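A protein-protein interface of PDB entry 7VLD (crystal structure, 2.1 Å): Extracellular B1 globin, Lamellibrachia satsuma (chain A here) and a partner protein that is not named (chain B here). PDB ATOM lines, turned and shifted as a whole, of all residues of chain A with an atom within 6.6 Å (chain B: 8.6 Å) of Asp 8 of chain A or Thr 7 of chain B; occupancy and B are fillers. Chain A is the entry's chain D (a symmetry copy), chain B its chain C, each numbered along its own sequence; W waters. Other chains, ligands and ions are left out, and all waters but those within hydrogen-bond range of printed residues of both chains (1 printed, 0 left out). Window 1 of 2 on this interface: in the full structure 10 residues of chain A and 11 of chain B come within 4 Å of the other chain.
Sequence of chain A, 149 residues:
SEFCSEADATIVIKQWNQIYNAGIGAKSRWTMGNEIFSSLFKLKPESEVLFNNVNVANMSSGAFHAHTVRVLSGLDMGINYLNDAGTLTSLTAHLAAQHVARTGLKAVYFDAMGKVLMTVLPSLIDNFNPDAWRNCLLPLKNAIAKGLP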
ATOM      1  N   CYS A   4      -1.740 -11.817 -14.512  1.00  0.00           N
ATOM      2  CA  CYS A   4      -2.394 -11.372 -15.736  1.00  0.00           C
ATOM      3  C   CYS A   4      -3.529 -10.417 -15.395  1.00  0.00           C
ATOM      4  O   CYS A   4      -3.939 -10.287 -14.239  1.00  0.00           O
ATOM      5  CB  CYS A   4      -2.905 -12.552 -16.582  1.00  0.00           C
ATOM      6  SG  CYS A   4      -4.260 -13.523 -15.877  1.00  0.00           S
ATOM      7  N   SER A   5      -4.033  -9.742 -16.426  1.00  0.00           N
ATOM      8  CA  SER A   5      -5.035  -8.706 -16.239  1.00  0.00           C
ATOM      9  C   SER A   5      -6.367  -9.316 -15.806  1.00  0.00           C
ATOM     10  O   SER A   5      -6.600 -10.523 -15.913  1.00  0.00           O
ATOM     11  CB  SER A   5      -5.223  -7.896 -17.522  1.00  0.00           C
ATOM     12  OG  SER A   5      -6.193  -8.494 -18.366  1.00  0.00           O
ATOM     13  N   GLU A   6      -7.253  -8.450 -15.314  1.00  0.00           N
ATOM     14  CA  GLU A   6      -8.553  -8.908 -14.838  1.00  0.00           C
ATOM     15  C   GLU A   6      -9.416  -9.422 -15.984  1.00  0.00           C
ATOM     16  O   GLU A   6     -10.147 -10.406 -15.823  1.00  0.00           O
ATOM     17  CB  GLU A   6      -9.260  -7.779 -14.089  1.00  0.00           C
ATOM     18  CG  GLU A   6     -10.670  -8.114 -13.640  1.00  0.00           C
ATOM     19  CD  GLU A   6     -11.325  -6.974 -12.887  1.00  0.00           C
ATOM     20  OE1 GLU A   6     -10.631  -6.313 -12.085  1.00  0.00           O
ATOM     21  OE2 GLU A   6     -12.530  -6.733 -13.104  1.00  0.00           O
ATOM     22  N   ALA A   7      -9.344  -8.776 -17.151  1.00  0.00           N
ATOM     23  CA  ALA A   7     -10.141  -9.232 -18.287  1.00  0.00           C
ATOM     24  C   ALA A   7      -9.589 -10.527 -18.868  1.00  0.00           C
ATOM     25  O   ALA A   7     -10.357 -11.397 -19.296  1.00  0.00           O
ATOM     26  CB  ALA A   7     -10.209  -8.146 -19.361  1.00  0.00           C
ATOM     27  N   ASP A   8      -8.262 -10.670 -18.903  1.00  0.00           N
ATOM     28  CA  ASP A   8      -7.674 -11.932 -19.342  1.00  0.00           C
ATOM     29  C   ASP A   8      -8.002 -13.056 -18.368  1.00  0.00           C
ATOM     30  O   ASP A   8      -8.321 -14.175 -18.786  1.00  0.00           O
ATOM     31  CB  ASP A   8      -6.159 -11.788 -19.500  1.00  0.00           C
ATOM     32  CG  ASP A   8      -5.772 -10.964 -20.715  1.00  0.00           C
ATOM     33  OD1 ASP A   8      -6.622 -10.790 -21.613  1.00  0.00           O
ATOM     34  OD2 ASP A   8      -4.615 -10.500 -20.775  1.00  0.00           O
ATOM     35  N   ALA A   9      -7.931 -12.776 -17.064  1.00  0.00           N
ATOM     36  CA  ALA A   9      -8.251 -13.791 -16.066  1.00  0.00           C
ATOM     37  C   ALA A   9      -9.710 -14.221 -16.162  1.00  0.00           C
ATOM     38  O   ALA A   9     -10.025 -15.407 -16.017  1.00  0.00           O
ATOM     39  CB  ALA A   9      -7.937 -13.267 -14.665  1.00  0.00           C
ATOM     40  N   THR A  10     -10.613 -13.267 -16.409  1.00  0.00           N
ATOM     41  CA  THR A  10     -12.029 -13.597 -16.545  1.00  0.00           C
ATOM     42  C   THR A  10     -12.262 -14.565 -17.700  1.00  0.00           C
ATOM     43  O   THR A  10     -13.098 -15.471 -17.602  1.00  0.00           O
ATOM     44  CB  THR A  10     -12.845 -12.317 -16.738  1.00  0.00           C
ATOM     45  OG1 THR A  10     -12.717 -11.486 -15.578  1.00  0.00           O
ATOM     46  CG2 THR A  10     -14.317 -12.640 -16.962  1.00  0.00           C
ATOM     47  N   ILE A  11     -11.523 -14.396 -18.796  1.00  0.00           N
ATOM     48  CA  ILE A  11     -11.655 -15.299 -19.935  1.00  0.00           C
ATOM     49  C   ILE A  11     -11.142 -16.688 -19.574  1.00  0.00           C
ATOM     50  O   ILE A  11     -11.796 -17.701 -19.849  1.00  0.00           O
ATOM     51  CB  ILE A  11     -10.921 -14.727 -21.161  1.00  0.00           C
ATOM     52  CG1 ILE A  11     -11.595 -13.438 -21.637  1.00  0.00           C
ATOM     53  CG2 ILE A  11     -10.865 -15.754 -22.283  1.00  0.00           C
ATOM     54  CD1 ILE A  11     -10.882 -12.771 -22.792  1.00  0.00           C
ATOM     55  N   VAL A  12      -9.963 -16.755 -18.950  1.00  0.00           N
ATOM     56  CA  VAL A  12      -9.385 -18.043 -18.575  1.00  0.00           C
ATOM     57  C   VAL A  12     -10.290 -18.771 -17.590  1.00  0.00           C
ATOM     58  O   VAL A  12     -10.530 -19.978 -17.720  1.00  0.00           O
ATOM     59  CB  VAL A  12      -7.969 -17.845 -18.001  1.00  0.00           C
ATOM     60  CG1 VAL A  12      -7.396 -19.171 -17.519  1.00  0.00           C
ATOM     61  CG2 VAL A  12      -7.060 -17.210 -19.041  1.00  0.00           C
ATOM     62  N   ILE A  13     -10.815 -18.050 -16.596  1.00  0.00           N
ATOM     63  CA  ILE A  13     -11.656 -18.678 -15.580  1.00  0.00           C
ATOM     64  C   ILE A  13     -12.941 -19.216 -16.200  1.00  0.00           C
ATOM     65  O   ILE A  13     -13.364 -20.340 -15.905  1.00  0.00           O
ATOM     66  CB  ILE A  13     -11.941 -17.684 -14.437  1.00  0.00           C
ATOM     67  CG1 ILE A  13     -10.659 -17.405 -13.646  1.00  0.00           C
ATOM     68  CG2 ILE A  13     -13.032 -18.218 -13.517  1.00  0.00           C
ATOM     69  CD1 ILE A  13     -10.775 -16.257 -12.664  1.00  0.00           C
ATOM     70  N   LEU A  82      -6.773 -16.089  -9.892  1.00  0.00           N
ATOM     71  CA  LEU A  82      -5.993 -15.206 -10.750  1.00  0.00           C
ATOM     72  C   LEU A  82      -6.215 -13.737 -10.408  1.00  0.00           C
ATOM     73  O   LEU A  82      -5.294 -12.925 -10.551  1.00  0.00           O
ATOM     74  CB  LEU A  82      -6.331 -15.465 -12.220  1.00  0.00           C
ATOM     75  CG  LEU A  82      -5.722 -16.707 -12.876  1.00  0.00           C
ATOM     76  CD1 LEU A  82      -6.366 -16.969 -14.231  1.00  0.00           C
ATOM     77  CD2 LEU A  82      -4.214 -16.563 -13.017  1.00  0.00           C
ATOM     78  N   ASN A 129      -8.892 -19.309 -26.167  1.00  0.00           N
ATOM     79  CA  ASN A 129      -8.163 -18.066 -26.376  1.00  0.00           C
ATOM     80  C   ASN A 129      -6.705 -18.276 -25.992  1.00  0.00           C
ATOM     81  O   ASN A 129      -6.343 -18.114 -24.819  1.00  0.00           O
ATOM     82  CB  ASN A 129      -8.792 -16.932 -25.559  1.00  0.00           C
ATOM     83  CG  ASN A 129      -8.210 -15.566 -25.891  1.00  0.00           C
ATOM     84  OD1 ASN A 129      -6.998 -15.409 -26.036  1.00  0.00           O
ATOM     85  ND2 ASN A 129      -9.078 -14.568 -26.003  1.00  0.00           N
ATOM     86  N   ASP A 131      -4.179 -16.460 -26.369  1.00  0.00           N
ATOM     87  CA  ASP A 131      -3.517 -15.260 -25.869  1.00  0.00           C
ATOM     88  C   ASP A 131      -3.819 -15.035 -24.392  1.00  0.00           C
ATOM     89  O   ASP A 131      -2.900 -14.865 -23.584  1.00  0.00           O
ATOM     90  CB  ASP A 131      -3.936 -14.041 -26.693  1.00  0.00           C
ATOM     91  CG  ASP A 131      -3.151 -13.912 -27.986  1.00  0.00           C
ATOM     92  OD1 ASP A 131      -2.291 -14.777 -28.255  1.00  0.00           O
ATOM     93  OD2 ASP A 131      -3.393 -12.941 -28.736  1.00  0.00           O
ATOM     94  N   ALA A 132      -5.102 -15.028 -24.024  1.00  0.00           N
ATOM     95  CA  ALA A 132      -5.469 -14.858 -22.622  1.00  0.00           C
ATOM     96  C   ALA A 132      -4.897 -15.978 -21.764  1.00  0.00           C
ATOM     97  O   ALA A 132      -4.412 -15.734 -20.652  1.00  0.00           O
ATOM     98  CB  ALA A 132      -6.991 -14.796 -22.480  1.00  0.00           C
ATOM     99  N   TRP A 133      -4.933 -17.213 -22.267  1.00  0.00           N
ATOM    100  CA  TRP A 133      -4.362 -18.328 -21.517  1.00  0.00           C
ATOM    101  C   TRP A 133      -2.854 -18.179 -21.367  1.00  0.00           C
ATOM    102  O   TRP A 133      -2.307 -18.437 -20.289  1.00  0.00           O
ATOM    103  CB  TRP A 133      -4.715 -19.652 -22.194  1.00  0.00           C
ATOM    104  CG  TRP A 133      -6.058 -20.169 -21.783  1.00  0.00           C
ATOM    105  CD1 TRP A 133      -7.263 -19.865 -22.343  1.00  0.00           C
ATOM    106  CD2 TRP A 133      -6.331 -21.073 -20.706  1.00  0.00           C
ATOM    107  NE1 TRP A 133      -8.270 -20.527 -21.687  1.00  0.00           N
ATOM    108  CE2 TRP A 133      -7.725 -21.276 -20.677  1.00  0.00           C
ATOM    109  CE3 TRP A 133      -5.533 -21.732 -19.767  1.00  0.00           C
ATOM    110  CZ2 TRP A 133      -8.337 -22.111 -19.745  1.00  0.00           C
ATOM    111  CZ3 TRP A 133      -6.144 -22.560 -18.842  1.00  0.00           C
ATOM    112  CH2 TRP A 133      -7.531 -22.744 -18.839  1.00  0.00           C
ATOM    113  N   ASN A 135      -1.149 -15.360 -21.343  1.00  0.00           N
ATOM    114  CA  ASN A 135      -0.875 -14.255 -20.432  1.00  0.00           C
ATOM    115  C   ASN A 135      -1.051 -14.662 -18.976  1.00  0.00           C
ATOM    116  O   ASN A 135      -0.357 -14.135 -18.100  1.00  0.00           O
ATOM    117  CB  ASN A 135      -1.784 -13.066 -20.752  1.00  0.00           C
ATOM    118  CG  ASN A 135      -1.547 -12.504 -22.140  1.00  0.00           C
ATOM    119  OD1 ASN A 135      -0.543 -12.806 -22.784  1.00  0.00           O
ATOM    120  ND2 ASN A 135      -2.472 -11.673 -22.604  1.00  0.00           N
ATOM    121  N   CYS A 136      -1.970 -15.583 -18.693  1.00  0.00           N
ATOM    122  CA  CYS A 136      -2.239 -16.006 -17.324  1.00  0.00           C
ATOM    123  C   CYS A 136      -1.464 -17.250 -16.915  1.00  0.00           C
ATOM    124  O   CYS A 136      -0.999 -17.333 -15.776  1.00  0.00           O
ATOM    125  CB  CYS A 136      -3.736 -16.259 -17.126  1.00  0.00           C
ATOM    126  SG  CYS A 136      -4.789 -14.800 -17.371  1.00  0.00           S
ATOM    127  N   SER B   2       3.555  -5.716 -16.761  1.00  0.00           N
ATOM    128  CA  SER B   2       3.946  -6.618 -17.838  1.00  0.00           C
ATOM    129  C   SER B   2       3.772  -5.953 -19.201  1.00  0.00           C
ATOM    130  O   SER B   2       3.057  -4.960 -19.330  1.00  0.00           O
ATOM    131  CB  SER B   2       3.132  -7.912 -17.772  1.00  0.00           C
ATOM    132  OG  SER B   2       3.499  -8.802 -18.813  1.00  0.00           O
ATOM    133  N   SER B   4       2.552  -7.622 -21.862  1.00  0.00           N
ATOM    134  CA  SER B   4       1.633  -8.433 -22.648  1.00  0.00           C
ATOM    135  C   SER B   4       0.490  -7.586 -23.196  1.00  0.00           C
ATOM    136  O   SER B   4      -0.007  -6.674 -22.529  1.00  0.00           O
ATOM    137  CB  SER B   4       1.073  -9.577 -21.801  1.00  0.00           C
ATOM    138  OG  SER B   4       2.061 -10.557 -21.543  1.00  0.00           O
ATOM    139  N   CYS B   5       0.077  -7.895 -24.423  1.00  0.00           N
ATOM    140  CA  CYS B   5      -1.103  -7.283 -25.030  1.00  0.00           C
ATOM    141  C   CYS B   5      -2.335  -7.926 -24.407  1.00  0.00           C
ATOM    142  O   CYS B   5      -2.737  -9.028 -24.786  1.00  0.00           O
ATOM    143  CB  CYS B   5      -1.080  -7.455 -26.545  1.00  0.00           C
ATOM    144  SG  CYS B   5      -2.643  -7.103 -27.400  1.00  0.00           S
ATOM    145  N   THR B   6      -2.934  -7.239 -23.438  1.00  0.00           N
ATOM    146  CA  THR B   6      -4.063  -7.778 -22.700  1.00  0.00           C
ATOM    147  C   THR B   6      -5.363  -7.583 -23.479  1.00  0.00           C
ATOM    148  O   THR B   6      -5.404  -6.934 -24.528  1.00  0.00           O
ATOM    149  CB  THR B   6      -4.174  -7.112 -21.330  1.00  0.00           C
ATOM    150  OG1 THR B   6      -4.602  -5.753 -21.491  1.00  0.00           O
ATOM    151  CG2 THR B   6      -2.828  -7.127 -20.623  1.00  0.00           C
ATOM    152  N   THR B   7      -6.441  -8.165 -22.943  1.00  0.00           N
ATOM    153  CA  THR B   7      -7.766  -7.933 -23.509  1.00  0.00           C
ATOM    154  C   THR B   7      -8.125  -6.454 -23.464  1.00  0.00           C
ATOM    155  O   THR B   7      -8.687  -5.913 -24.424  1.00  0.00           O
ATOM    156  CB  THR B   7      -8.814  -8.759 -22.758  1.00  0.00           C
ATOM    157  OG1 THR B   7      -8.477 -10.149 -22.833  1.00  0.00           O
ATOM    158  CG2 THR B   7     -10.200  -8.544 -23.354  1.00  0.00           C
ATOM    159  N   GLU B   8      -7.803  -5.783 -22.355  1.00  0.00           N
ATOM    160  CA  GLU B   8      -8.038  -4.346 -22.257  1.00  0.00           C
ATOM    161  C   GLU B   8      -7.273  -3.595 -23.338  1.00  0.00           C
ATOM    162  O   GLU B   8      -7.833  -2.735 -24.029  1.00  0.00           O
ATOM    163  CB  GLU B   8      -7.637  -3.840 -20.869  1.00  0.00           C
ATOM    164  CG  GLU B   8      -8.452  -4.408 -19.717  1.00  0.00           C
ATOM    165  CD  GLU B   8      -7.857  -5.677 -19.141  1.00  0.00           C
ATOM    166  OE1 GLU B   8      -7.008  -6.302 -19.811  1.00  0.00           O
ATOM    167  OE2 GLU B   8      -8.238  -6.050 -18.010  1.00  0.00           O
ATOM    168  N   ASP B   9      -5.985  -3.912 -23.499  1.00  0.00           N
ATOM    169  CA  ASP B   9      -5.181  -3.278 -24.538  1.00  0.00           C
ATOM    170  C   ASP B   9      -5.758  -3.536 -25.924  1.00  0.00           C
ATOM    171  O   ASP B   9      -5.704  -2.663 -26.799  1.00  0.00           O
ATOM    172  CB  ASP B   9      -3.738  -3.779 -24.467  1.00  0.00           C
ATOM    173  CG  ASP B   9      -3.004  -3.289 -23.235  1.00  0.00           C
ATOM    174  OD1 ASP B   9      -3.384  -2.231 -22.692  1.00  0.00           O
ATOM    175  OD2 ASP B   9      -2.036  -3.960 -22.817  1.00  0.00           O
ATOM    176  N   ARG B  10      -6.307  -4.735 -26.146  1.00  0.00           N
ATOM    177  CA  ARG B  10      -6.899  -5.050 -27.444  1.00  0.00           C
ATOM    178  C   ARG B  10      -8.099  -4.160 -27.732  1.00  0.00           C
ATOM    179  O   ARG B  10      -8.269  -3.679 -28.859  1.00  0.00           O
ATOM    180  CB  ARG B  10      -7.293  -6.526 -27.494  1.00  0.00           C
ATOM    181  CG  ARG B  10      -6.117  -7.466 -27.692  1.00  0.00           C
ATOM    182  CD  ARG B  10      -6.308  -8.793 -26.970  1.00  0.00           C
ATOM    183  NE  ARG B  10      -5.021  -9.376 -26.599  1.00  0.00           N
ATOM    184  CZ  ARG B  10      -4.421 -10.362 -27.258  1.00  0.00           C
ATOM    185  NH1 ARG B  10      -4.996 -10.898 -28.326  1.00  0.00           N
ATOM    186  NH2 ARG B  10      -3.246 -10.817 -26.843  1.00  0.00           N
ATOM    187  N   ARG B  11      -8.944  -3.928 -26.724  1.00  0.00           N
ATOM    188  CA  ARG B  11     -10.083  -3.034 -26.906  1.00  0.00           C
ATOM    189  C   ARG B  11      -9.626  -1.611 -27.204  1.00  0.00           C
ATOM    190  O   ARG B  11     -10.248  -0.908 -28.010  1.00  0.00           O
ATOM    191  CB  ARG B  11     -10.976  -3.061 -25.665  1.00  0.00           C
ATOM    192  CG  ARG B  11     -11.584  -4.422 -25.348  1.00  0.00           C
ATOM    193  CD  ARG B  11     -12.608  -4.318 -24.222  1.00  0.00           C
ATOM    194  NE  ARG B  11     -13.308  -5.579 -23.988  1.00  0.00           N
ATOM    195  CZ  ARG B  11     -13.141  -6.343 -22.913  1.00  0.00           C
ATOM    196  NH1 ARG B  11     -12.298  -5.976 -21.956  1.00  0.00           N
ATOM    197  NH2 ARG B  11     -13.823  -7.473 -22.789  1.00  0.00           N
ATOM    198  N   GLU B  12      -8.537  -1.167 -26.569  1.00  0.00           N
ATOM    199  CA  GLU B  12      -8.064   0.195 -26.795  1.00  0.00           C
ATOM    200  C   GLU B  12      -7.493   0.362 -28.197  1.00  0.00           C
ATOM    201  O   GLU B  12      -7.722   1.390 -28.845  1.00  0.00           O
ATOM    202  CB  GLU B  12      -7.016   0.579 -25.750  1.00  0.00           C
ATOM    203  CG  GLU B  12      -7.583   0.917 -24.385  1.00  0.00           C
ATOM    204  CD  GLU B  12      -6.584   1.660 -23.519  1.00  0.00           C
ATOM    205  OE1 GLU B  12      -5.992   2.646 -24.006  1.00  0.00           O
ATOM    206  OE2 GLU B  12      -6.382   1.251 -22.356  1.00  0.00           O
ATOM    207  N   MET B  13      -6.741  -0.629 -28.682  1.00  0.00           N
ATOM    208  CA  MET B  13      -6.163  -0.519 -30.017  1.00  0.00           C
ATOM    209  C   MET B  13      -7.246  -0.503 -31.087  1.00  0.00           C
ATOM    210  O   MET B  13      -7.140   0.233 -32.076  1.00  0.00           O
ATOM    211  CB  MET B  13      -5.178  -1.659 -30.271  1.00  0.00           C
ATOM    212  CG  MET B  13      -4.291  -1.435 -31.485  1.00  0.00           C
ATOM    213  SD  MET B  13      -3.241  -2.843 -31.878  1.00  0.00           S
ATOM    214  CE  MET B  13      -2.051  -2.086 -32.984  1.00  0.00           C
ATOM    215  N   GLN B  14      -8.297  -1.306 -30.907  1.00  0.00           N
ATOM    216  CA  GLN B  14      -9.374  -1.339 -31.888  1.00  0.00           C
ATOM    217  C   GLN B  14     -10.165  -0.036 -31.899  1.00  0.00           C
ATOM    218  O   GLN B  14     -10.672   0.368 -32.950  1.00  0.00           O
ATOM    219  CB  GLN B  14     -10.287  -2.537 -31.616  1.00  0.00           C
ATOM    220  CG  GLN B  14      -9.617  -3.878 -31.892  1.00  0.00           C
ATOM    221  CD  GLN B  14     -10.375  -5.059 -31.311  1.00  0.00           C
ATOM    222  OE1 GLN B  14     -11.242  -4.898 -30.453  1.00  0.00           O
ATOM    223  NE2 GLN B  14     -10.044  -6.259 -31.778  1.00  0.00           N
ATOM    224  N   LEU B  82      -7.365  -9.623 -33.195  1.00  0.00           N
ATOM    225  CA  LEU B  82      -6.950  -9.666 -31.796  1.00  0.00           C
ATOM    226  C   LEU B  82      -8.058 -10.221 -30.911  1.00  0.00           C
ATOM    227  O   LEU B  82      -7.781 -10.768 -29.837  1.00  0.00           O
ATOM    228  CB  LEU B  82      -6.540  -8.270 -31.320  1.00  0.00           C
ATOM    229  CG  LEU B  82      -5.260  -7.659 -31.893  1.00  0.00           C
ATOM    230  CD1 LEU B  82      -5.151  -6.196 -31.497  1.00  0.00           C
ATOM    231  CD2 LEU B  82      -4.036  -8.431 -31.426  1.00  0.00           C
ATOM    232  N   SER B  83      -9.315 -10.093 -31.347  1.00  0.00           N
ATOM    233  CA  SER B  83     -10.438 -10.648 -30.602  1.00  0.00           C
ATOM    234  C   SER B  83     -10.530 -12.164 -30.727  1.00  0.00           C
ATOM    235  O   SER B  83     -11.168 -12.802 -29.885  1.00  0.00           O
ATOM    236  CB  SER B  83     -11.746 -10.010 -31.076  1.00  0.00           C
ATOM    237  OG  SER B  83     -11.741  -8.610 -30.858  1.00  0.00           O
ATOM    238  N   PRO B  85      -7.668 -14.791 -31.210  1.00  0.00           N
ATOM    239  CA  PRO B  85      -6.237 -15.067 -31.426  1.00  0.00           C
ATOM    240  C   PRO B  85      -5.939 -16.402 -32.091  1.00  0.00           C
ATOM    241  O   PRO B  85      -4.854 -16.545 -32.669  1.00  0.00           O
ATOM    242  CB  PRO B  85      -5.648 -15.008 -30.010  1.00  0.00           C
ATOM    243  CG  PRO B  85      -6.801 -15.249 -29.108  1.00  0.00           C
ATOM    244  CD  PRO B  85      -7.998 -14.658 -29.781  1.00  0.00           C
ATOM    245  N   ALA B 132      -0.645   1.197 -24.784  1.00  0.00           N
ATOM    246  CA  ALA B 132      -1.472   0.060 -25.172  1.00  0.00           C
ATOM    247  C   ALA B 132      -1.334  -0.265 -26.653  1.00  0.00           C
ATOM    248  O   ALA B 132      -1.413  -1.438 -27.036  1.00  0.00           O
ATOM    249  CB  ALA B 132      -2.936   0.327 -24.823  1.00  0.00           C
ATOM    250  N   CYS B 136       0.262  -4.211 -28.244  1.00  0.00           N
ATOM    251  CA  CYS B 136      -0.449  -5.072 -29.179  1.00  0.00           C
ATOM    252  C   CYS B 136       0.105  -4.988 -30.593  1.00  0.00           C
ATOM    253  O   CYS B 136       0.014  -5.967 -31.343  1.00  0.00           O
ATOM    254  CB  CYS B 136      -1.942  -4.737 -29.172  1.00  0.00           C
ATOM    255  SG  CYS B 136      -2.725  -5.079 -27.578  1.00  0.00           S
HETATM  256  O   HOH W   1      -0.824 -12.549 -25.593  1.00  0.00           O
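Water W1 bridges the side-chain amide oxygen (OD1) of Asn 135 of chain A (2.8 Å) and the guanidinium group (NH2) of Arg 10 of chain B (3.2 Å).
The side-chain sulfur of Cys 136 of chain B forms a disulfide with the side-chain sulfur of Cys 5 of chain B. OG1 of Thr 6 of chain B is in hydrogen-bond range of OE1 of Glu 8 of chain B, 3.0 Å away. The guanidinium group (NH1) of Arg 10 of chain B is in hydrogen-bond range of the backbone carbonyl oxygen (O) of Leu 82 of chain B, at 3.2 Å. O of Cys 5 of chain B is in hydrogen-bond range of NH2 of Arg 10 of chain B (2.8 Å). The side-chain hydroxyl of Thr 6 of chain B sits at hydrogen-bond distance from the backbone NH of Asp 9 of chain B, at 3.1 Å. The side-chain hydroxyl (OG) of Ser 2 of chain B lies close to the backbone NH (N) of Ser 4 of chain B (3.4 Å).
The side-chain carboxylate (OE1) of Glu 8 of chain B is in hydrogen-bond range of the side-chain hydroxyl (OG) of Ser 5 of chain A. The backbone carbonyl oxygen of Cys 5 of chain B sits at hydrogen-bond distance from the side-chain amide nitrogen of Asn 135 of chain A (3.4 Å). The side-chain carboxylate of Glu 8 of chain B lies within hydrogen-bond range of the backbone NH of Ala 7 of chain A (3.1 Å). N of Thr 7 of chain B lies within hydrogen-bond range of OD1 of Asp 8 of chain A (2.9 Å). The guanidinium group (NH1) of Arg 10 of chain B is in salt-bridge range of the side-chain carboxylate (OD2) of Asp 131 of chain A (2.6 Å).
Of the 17 printed residues of chain B, 8 touch a printed residue of chain A. Hydrophobic or aromatic side chains of chain A that line the printed part of chain B: Ala 7 and Ile 11. Among the printed residues, Asp or Glu carboxylates within 4 Å of a Lys or Arg side-chain nitrogen of the other chain: Asp 131 of chain A with Arg 10 of chain B (2.6 Å).
Asp 8 of chain A touches just these residues of chain B: Thr 6 (3.4 Å) and Thr 7 (2.3 Å). Printed residues of chain B within 4 Å of Asp 131 of chain A: Arg 10 (2.6 Å) and Pro 85 (3.3 Å). Of the printed residues of chain A, Cys 5 of chain B touches Asn 135 (3.4 Å). Thr 7 of chain B touches three residues of chain A. Ala 132 of chain B touches none of the printed residues of chain A. The nearest residue of chain B that does not touch Asp 8 of chain A is Glu 8 of chain B (4.6 Å). The nearest printed residue of chain A that does not touch Ser 4 of chain B is Asp 8 of chain A (5.9 Å).
Ser 5 of chain A touches Thr 6 of chain B (OG to CB, 3.8 Å). Glu 6 of chain A touches Glu 8 of chain B. Ala 7 of chain A touches Thr 7 of chain B. Ala 7 of chain A touches Arg 11 of chain B (CB to NH1, 3.98 Å). Thr 6 of chain B touches Asp 8 of chain A (CA to OD2, 3.4 Å). OG1 of Thr 7 of chain B touches CD1 of Ile 11 of chain A, 3.6 Å away. Asn 129 of chain A touches Pro 85 of chain B. Pro 85 of chain B touches Asp 131 of chain A (CB to OD2, 3.3 Å). OG of Ser 4 of chain B touches OD1 of Asn 135 of chain A (3.7 Å).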
